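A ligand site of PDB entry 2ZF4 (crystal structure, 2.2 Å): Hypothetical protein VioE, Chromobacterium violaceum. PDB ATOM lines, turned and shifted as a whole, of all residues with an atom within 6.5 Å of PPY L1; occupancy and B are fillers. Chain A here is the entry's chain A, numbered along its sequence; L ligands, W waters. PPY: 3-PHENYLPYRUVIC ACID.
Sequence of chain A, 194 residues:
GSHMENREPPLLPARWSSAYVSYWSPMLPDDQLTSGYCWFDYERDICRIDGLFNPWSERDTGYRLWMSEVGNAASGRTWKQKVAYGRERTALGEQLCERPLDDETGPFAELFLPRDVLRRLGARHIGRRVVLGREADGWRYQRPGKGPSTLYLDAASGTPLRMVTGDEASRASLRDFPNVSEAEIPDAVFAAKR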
ATOM      1  N   TYR A  20       9.722  11.590  14.036  1.00  0.00           N
ATOM      2  CA  TYR A  20      10.435  10.386  14.432  1.00  0.00           C
ATOM      3  C   TYR A  20      11.763  10.767  15.056  1.00  0.00           C
ATOM      4  O   TYR A  20      12.352  11.827  14.739  1.00  0.00           O
ATOM      5  CB  TYR A  20      10.643   9.436  13.217  1.00  0.00           C
ATOM      6  CG  TYR A  20      11.695   9.962  12.256  1.00  0.00           C
ATOM      7  CD1 TYR A  20      13.049   9.682  12.451  1.00  0.00           C
ATOM      8  CD2 TYR A  20      11.326  10.765  11.182  1.00  0.00           C
ATOM      9  CE1 TYR A  20      14.000  10.181  11.614  1.00  0.00           C
ATOM     10  CE2 TYR A  20      12.278  11.256  10.304  1.00  0.00           C
ATOM     11  CZ  TYR A  20      13.608  10.967  10.524  1.00  0.00           C
ATOM     12  OH  TYR A  20      14.524  11.487   9.674  1.00  0.00           O
ATOM     13  N   VAL A  21      12.235   9.912  15.948  1.00  0.00           N
ATOM     14  CA  VAL A  21      13.554  10.029  16.534  1.00  0.00           C
ATOM     15  C   VAL A  21      14.251   8.713  16.183  1.00  0.00           C
ATOM     16  O   VAL A  21      13.682   7.634  16.369  1.00  0.00           O
ATOM     17  CB  VAL A  21      13.509  10.205  18.072  1.00  0.00           C
ATOM     18  CG1 VAL A  21      14.889  10.386  18.623  1.00  0.00           C
ATOM     19  CG2 VAL A  21      12.629  11.399  18.463  1.00  0.00           C
ATOM     20  N   SER A  22      15.471   8.796  15.661  1.00  0.00           N
ATOM     21  CA  SER A  22      16.127   7.648  15.087  1.00  0.00           C
ATOM     22  C   SER A  22      17.461   7.470  15.787  1.00  0.00           C
ATOM     23  O   SER A  22      18.198   8.435  15.962  1.00  0.00           O
ATOM     24  CB  SER A  22      16.349   7.881  13.589  1.00  0.00           C
ATOM     25  OG  SER A  22      16.842   6.704  12.976  1.00  0.00           O
ATOM     26  N   TYR A  23      17.760   6.231  16.185  1.00  0.00           N
ATOM     27  CA  TYR A  23      18.975   5.919  16.935  1.00  0.00           C
ATOM     28  C   TYR A  23      19.310   4.433  16.865  1.00  0.00           C
ATOM     29  O   TYR A  23      18.777   3.704  16.014  1.00  0.00           O
ATOM     30  CB  TYR A  23      18.881   6.410  18.395  1.00  0.00           C
ATOM     31  CG  TYR A  23      17.684   5.910  19.183  1.00  0.00           C
ATOM     32  CD1 TYR A  23      16.411   6.457  18.978  1.00  0.00           C
ATOM     33  CD2 TYR A  23      17.828   4.927  20.163  1.00  0.00           C
ATOM     34  CE1 TYR A  23      15.312   6.023  19.706  1.00  0.00           C
ATOM     35  CE2 TYR A  23      16.725   4.470  20.888  1.00  0.00           C
ATOM     36  CZ  TYR A  23      15.477   5.027  20.647  1.00  0.00           C
ATOM     37  OH  TYR A  23      14.370   4.603  21.345  1.00  0.00           O
ATOM     38  N   THR A  34      19.096  11.314  15.819  1.00  0.00           N
ATOM     39  CA  THR A  34      18.559  12.277  14.877  1.00  0.00           C
ATOM     40  C   THR A  34      17.032  12.341  14.989  1.00  0.00           C
ATOM     41  O   THR A  34      16.409  11.503  15.640  1.00  0.00           O
ATOM     42  CB  THR A  34      18.988  11.976  13.418  1.00  0.00           C
ATOM     43  OG1 THR A  34      18.508  10.694  13.007  1.00  0.00           O
ATOM     44  CG2 THR A  34      20.532  12.025  13.259  1.00  0.00           C
ATOM     45  N   ILE A  49       9.857  11.166   3.971  1.00  0.00           N
ATOM     46  CA  ILE A  49      10.644  11.303   5.208  1.00  0.00           C
ATOM     47  C   ILE A  49      11.599  12.479   5.072  1.00  0.00           C
ATOM     48  O   ILE A  49      12.338  12.542   4.096  1.00  0.00           O
ATOM     49  CB  ILE A  49      11.453  10.019   5.509  1.00  0.00           C
ATOM     50  CG1 ILE A  49      10.548   8.779   5.371  1.00  0.00           C
ATOM     51  CG2 ILE A  49      12.074  10.094   6.937  1.00  0.00           C
ATOM     52  CD1 ILE A  49      11.290   7.467   5.393  1.00  0.00           C
ATOM     53  N   ASP A  50      11.553  13.410   6.026  1.00  0.00           N
ATOM     54  CA  ASP A  50      12.486  14.557   6.107  1.00  0.00           C
ATOM     55  C   ASP A  50      13.327  14.457   7.379  1.00  0.00           C
ATOM     56  O   ASP A  50      12.773  14.445   8.481  1.00  0.00           O
ATOM     57  CB  ASP A  50      11.743  15.896   6.158  1.00  0.00           C
ATOM     58  CG  ASP A  50      11.021  16.212   4.866  1.00  0.00           C
ATOM     59  OD1 ASP A  50      10.841  15.276   4.050  1.00  0.00           O
ATOM     60  OD2 ASP A  50      10.656  17.398   4.677  1.00  0.00           O
ATOM     61  N   GLY A  51      14.645  14.447   7.219  1.00  0.00           N
ATOM     62  CA  GLY A  51      15.556  14.438   8.369  1.00  0.00           C
ATOM     63  C   GLY A  51      17.017  14.349   7.969  1.00  0.00           C
ATOM     64  O   GLY A  51      17.350  14.117   6.797  1.00  0.00           O
ATOM     65  N   LEU A  52      17.891  14.527   8.959  1.00  0.00           N
ATOM     66  CA  LEU A  52      19.300  14.251   8.797  1.00  0.00           C
ATOM     67  C   LEU A  52      19.440  12.742   8.613  1.00  0.00           C
ATOM     68  O   LEU A  52      19.068  11.981   9.493  1.00  0.00           O
ATOM     69  CB  LEU A  52      20.057  14.693  10.040  1.00  0.00           C
ATOM     70  CG  LEU A  52      21.024  15.868  10.181  1.00  0.00           C
ATOM     71  CD1 LEU A  52      21.209  16.746   8.977  1.00  0.00           C
ATOM     72  CD2 LEU A  52      20.813  16.697  11.494  1.00  0.00           C
ATOM     73  N   PHE A  53      19.926  12.305   7.464  1.00  0.00           N
ATOM     74  CA  PHE A  53      20.029  10.870   7.241  1.00  0.00           C
ATOM     75  C   PHE A  53      20.834  10.129   8.329  1.00  0.00           C
ATOM     76  O   PHE A  53      21.903  10.587   8.738  1.00  0.00           O
ATOM     77  CB  PHE A  53      20.579  10.550   5.850  1.00  0.00           C
ATOM     78  CG  PHE A  53      20.233   9.166   5.399  1.00  0.00           C
ATOM     79  CD1 PHE A  53      18.985   8.901   4.839  1.00  0.00           C
ATOM     80  CD2 PHE A  53      21.117   8.120   5.593  1.00  0.00           C
ATOM     81  CE1 PHE A  53      18.647   7.600   4.439  1.00  0.00           C
ATOM     82  CE2 PHE A  53      20.785   6.820   5.214  1.00  0.00           C
ATOM     83  CZ  PHE A  53      19.551   6.561   4.627  1.00  0.00           C
ATOM     84  N   ASN A  54      20.293   9.003   8.780  1.00  0.00           N
ATOM     85  CA  ASN A  54      20.861   8.159   9.820  1.00  0.00           C
ATOM     86  C   ASN A  54      20.708   6.699   9.361  1.00  0.00           C
ATOM     87  O   ASN A  54      19.603   6.240   9.150  1.00  0.00           O
ATOM     88  CB  ASN A  54      20.084   8.402  11.127  1.00  0.00           C
ATOM     89  CG  ASN A  54      20.789   7.864  12.363  1.00  0.00           C
ATOM     90  OD1 ASN A  54      21.699   7.051  12.270  1.00  0.00           O
ATOM     91  ND2 ASN A  54      20.371   8.341  13.537  1.00  0.00           N
ATOM     92  N   PRO A  55      21.818   5.954   9.174  1.00  0.00           N
ATOM     93  CA  PRO A  55      23.206   6.300   9.418  1.00  0.00           C
ATOM     94  C   PRO A  55      23.858   6.967   8.216  1.00  0.00           C
ATOM     95  O   PRO A  55      23.454   6.746   7.051  1.00  0.00           O
ATOM     96  CB  PRO A  55      23.864   4.959   9.709  1.00  0.00           C
ATOM     97  CG  PRO A  55      23.086   3.973   8.885  1.00  0.00           C
ATOM     98  CD  PRO A  55      21.699   4.572   8.637  1.00  0.00           C
ATOM     99  N   TRP A  66      21.470  16.053   5.040  1.00  0.00           N
ATOM    100  CA  TRP A  66      20.035  16.210   5.308  1.00  0.00           C
ATOM    101  C   TRP A  66      19.328  15.795   4.035  1.00  0.00           C
ATOM    102  O   TRP A  66      19.779  16.110   2.938  1.00  0.00           O
ATOM    103  CB  TRP A  66      19.646  17.641   5.699  1.00  0.00           C
ATOM    104  CG  TRP A  66      18.131  17.836   5.766  1.00  0.00           C
ATOM    105  CD1 TRP A  66      17.332  17.665   6.844  1.00  0.00           C
ATOM    106  CD2 TRP A  66      17.260  18.199   4.679  1.00  0.00           C
ATOM    107  NE1 TRP A  66      16.020  17.923   6.521  1.00  0.00           N
ATOM    108  CE2 TRP A  66      15.939  18.242   5.198  1.00  0.00           C
ATOM    109  CE3 TRP A  66      17.472  18.516   3.331  1.00  0.00           C
ATOM    110  CZ2 TRP A  66      14.839  18.581   4.409  1.00  0.00           C
ATOM    111  CZ3 TRP A  66      16.367  18.832   2.548  1.00  0.00           C
ATOM    112  CH2 TRP A  66      15.063  18.868   3.100  1.00  0.00           C
ATOM    113  N   MET A  67      18.211  15.083   4.173  1.00  0.00           N
ATOM    114  CA  MET A  67      17.493  14.661   2.968  1.00  0.00           C
ATOM    115  C   MET A  67      15.970  14.700   3.160  1.00  0.00           C
ATOM    116  O   MET A  67      15.468  14.454   4.246  1.00  0.00           O
ATOM    117  CB  MET A  67      17.942  13.261   2.549  1.00  0.00           C
ATOM    118  CG  MET A  67      17.242  12.732   1.306  1.00  0.00           C
ATOM    119  SD  MET A  67      18.209  11.426   0.581  1.00  0.00           S
ATOM    120  CE  MET A  67      17.569   9.996   1.422  1.00  0.00           C
ATOM    121  N   SER A  68      15.263  15.041   2.086  1.00  0.00           N
ATOM    122  CA  SER A  68      13.829  14.776   2.007  1.00  0.00           C
ATOM    123  C   SER A  68      13.615  13.786   0.843  1.00  0.00           C
ATOM    124  O   SER A  68      13.952  14.078  -0.285  1.00  0.00           O
ATOM    125  CB  SER A  68      13.061  16.071   1.754  1.00  0.00           C
ATOM    126  OG  SER A  68      11.710  15.804   1.412  1.00  0.00           O
ATOM    127  N   GLU A  69      13.048  12.608   1.121  1.00  0.00           N
ATOM    128  CA  GLU A  69      12.812  11.592   0.115  1.00  0.00           C
ATOM    129  C   GLU A  69      11.316  11.353  -0.013  1.00  0.00           C
ATOM    130  O   GLU A  69      10.600  11.306   0.989  1.00  0.00           O
ATOM    131  CB  GLU A  69      13.563  10.286   0.475  1.00  0.00           C
ATOM    132  CG  GLU A  69      13.105   9.064  -0.323  1.00  0.00           C
ATOM    133  CD  GLU A  69      14.095   7.902  -0.276  1.00  0.00           C
ATOM    134  OE1 GLU A  69      14.914   7.834   0.670  1.00  0.00           O
ATOM    135  OE2 GLU A  69      14.025   7.048  -1.189  1.00  0.00           O
ATOM    136  N   PHE A 112       9.045   1.855   2.917  1.00  0.00           N
ATOM    137  CA  PHE A 112       9.997   1.580   3.995  1.00  0.00           C
ATOM    138  C   PHE A 112       9.390   0.712   5.112  1.00  0.00           C
ATOM    139  O   PHE A 112      10.092  -0.079   5.752  1.00  0.00           O
ATOM    140  CB  PHE A 112      10.541   2.904   4.562  1.00  0.00           C
ATOM    141  CG  PHE A 112      11.400   3.685   3.598  1.00  0.00           C
ATOM    142  CD1 PHE A 112      12.614   3.187   3.137  1.00  0.00           C
ATOM    143  CD2 PHE A 112      10.989   4.945   3.143  1.00  0.00           C
ATOM    144  CE1 PHE A 112      13.399   3.920   2.247  1.00  0.00           C
ATOM    145  CE2 PHE A 112      11.774   5.678   2.254  1.00  0.00           C
ATOM    146  CZ  PHE A 112      12.973   5.174   1.821  1.00  0.00           C
ATOM    147  N   SER A 173      18.707  -0.748  14.732  1.00  0.00           N
ATOM    148  CA  SER A 173      18.271   0.629  14.672  1.00  0.00           C
ATOM    149  C   SER A 173      16.892   0.741  15.332  1.00  0.00           C
ATOM    150  O   SER A 173      16.071  -0.194  15.269  1.00  0.00           O
ATOM    151  CB  SER A 173      18.252   1.130  13.235  1.00  0.00           C
ATOM    152  OG  SER A 173      16.948   1.222  12.744  1.00  0.00           O
ATOM    153  N   ARG A 175      13.637   3.437  15.554  1.00  0.00           N
ATOM    154  CA  ARG A 175      12.926   4.662  15.172  1.00  0.00           C
ATOM    155  C   ARG A 175      11.662   4.748  15.999  1.00  0.00           C
ATOM    156  O   ARG A 175      10.844   3.812  15.977  1.00  0.00           O
ATOM    157  CB  ARG A 175      12.592   4.670  13.665  1.00  0.00           C
ATOM    158  CG  ARG A 175      13.838   4.718  12.777  1.00  0.00           C
ATOM    159  CD  ARG A 175      13.531   4.331  11.366  1.00  0.00           C
ATOM    160  NE  ARG A 175      14.741   4.196  10.566  1.00  0.00           N
ATOM    161  CZ  ARG A 175      15.100   3.094   9.919  1.00  0.00           C
ATOM    162  NH1 ARG A 175      14.320   2.031   9.962  1.00  0.00           N
ATOM    163  NH2 ARG A 175      16.222   3.064   9.197  1.00  0.00           N
HETATM  164  C1  PPY L   1      16.559   7.271   9.571  1.00  0.00           C
HETATM  165  O1  PPY L   1      16.332   6.051   9.684  1.00  0.00           O
HETATM  166  O2  PPY L   1      16.796   7.962  10.585  1.00  0.00           O
HETATM  167  C2  PPY L   1      16.597   7.899   8.247  1.00  0.00           C
HETATM  168  O3  PPY L   1      17.605   8.513   7.940  1.00  0.00           O
HETATM  169  C3  PPY L   1      15.442   7.771   7.259  1.00  0.00           C
HETATM  170  C1' PPY L   1      15.401   8.845   6.152  1.00  0.00           C
HETATM  171  C2' PPY L   1      15.698  10.192   6.418  1.00  0.00           C
HETATM  172  C3' PPY L   1      15.642  11.153   5.399  1.00  0.00           C
HETATM  173  C4' PPY L   1      15.260  10.768   4.099  1.00  0.00           C
HETATM  174  C5' PPY L   1      14.951   9.427   3.831  1.00  0.00           C
HETATM  175  C6' PPY L   1      15.016   8.470   4.852  1.00  0.00           C
HETATM  176  C1  PPY L   2      14.050   1.934   6.480  1.00  0.00           C
HETATM  177  O1  PPY L   2      13.490   0.851   6.789  1.00  0.00           O
HETATM  178  O2  PPY L   2      15.111   1.934   5.803  1.00  0.00           O
HETATM  179  C2  PPY L   2      13.457   3.216   6.895  1.00  0.00           C
HETATM  180  O3  PPY L   2      14.033   4.261   6.615  1.00  0.00           O
HETATM  181  C3  PPY L   2      12.157   3.241   7.670  1.00  0.00           C
HETATM  182  C1' PPY L   2      11.731   4.578   8.239  1.00  0.00           C
HETATM  183  C2' PPY L   2      12.611   5.652   8.386  1.00  0.00           C
HETATM  184  C3' PPY L   2      12.174   6.860   8.940  1.00  0.00           C
HETATM  185  C4' PPY L   2      10.845   7.000   9.346  1.00  0.00           C
HETATM  186  C5' PPY L   2       9.964   5.925   9.208  1.00  0.00           C
HETATM  187  C6' PPY L   2      10.406   4.729   8.666  1.00  0.00           C
HETATM  188  O   HOH W   1      17.493   5.150   7.220  1.00  0.00           O
HETATM  189  O   HOH W   2      18.825   4.045  10.542  1.00  0.00           O
HETATM  190  O   HOH W   3      16.983  10.635  10.716  1.00  0.00           O
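O3 of PPY L1 is in hydrogen-bond range of N of Asn 54. The guanidinium group (NE) of Arg 175 lies within salt-bridge range of an oxygen (O1) of PPY L1 (2.6 Å). The side-chain hydroxyl (OG) of Ser 22 sits at hydrogen-bond distance from an oxygen (O2) of PPY L1 (2.7 Å). The guanidinium group (NH1) of Arg 175 lies within salt-bridge range of an oxygen (O1) of PPY L2, at 3.5 Å.
O of Gly 51 is in hydrogen-bond range of N of Met 67, at 2.9 Å. The backbone carbonyl oxygen of Ser 22 is in hydrogen-bond range of the side-chain amide nitrogen of Asn 54, 3.3 Å away. The side-chain hydroxyl (OG1) of Thr 34 sits at hydrogen-bond distance from the side-chain amide nitrogen (ND2) of Asn 54, at 3.0 Å. The backbone NH (N) of Glu 69 sits at hydrogen-bond distance from the backbone carbonyl oxygen (O) of Ile 49 (3.1 Å). The backbone NH of Ser 22 is in hydrogen-bond range of the backbone carbonyl oxygen of Thr 34.
Tyr 20 touches PPY L1. Ile 49 touches PPY L1. Gly 51 touches PPY L1. Phe 53 touches PPY L1 (CD1 to O3, 3.4 Å). O of Met 67 touches C3' of PPY L1, 3.5 Å away. Glu 69 touches PPY L1 (OE1 to C5', 3.5 Å). Hydrophobic or aromatic side chains that line PPY L1: Tyr 20, Ile 49, Phe 53 and Met 67. Nine residues have an atom within 4 Å of PPY L1: Tyr 20, Ser 22, Ile 49, Gly 51, Phe 53, Asn 54, Met 67, Glu 69 and Arg 175. The nearest printed residue that does not touch PPY L1 is Thr 34 (4.03 Å).
Water W3 lies within hydrogen-bond range of O2 of PPY L1 (2.7 Å), OG1 of Thr 34 (2.8 Å), O of Leu 52 (2.8 Å) and OH of Tyr 20 (2.8 Å). Water W1 lies within hydrogen-bond range of O1 of PPY L1 (2.9 Å), O of Asn 54 (3.1 Å) and NH2 of Arg 175 (3.1 Å). Water W2 lies within hydrogen-bond range of O of Asn 54 (2.7 Å), NH2 of Arg 175 (3.1 Å) and O1 of PPY L1 (3.3 Å).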
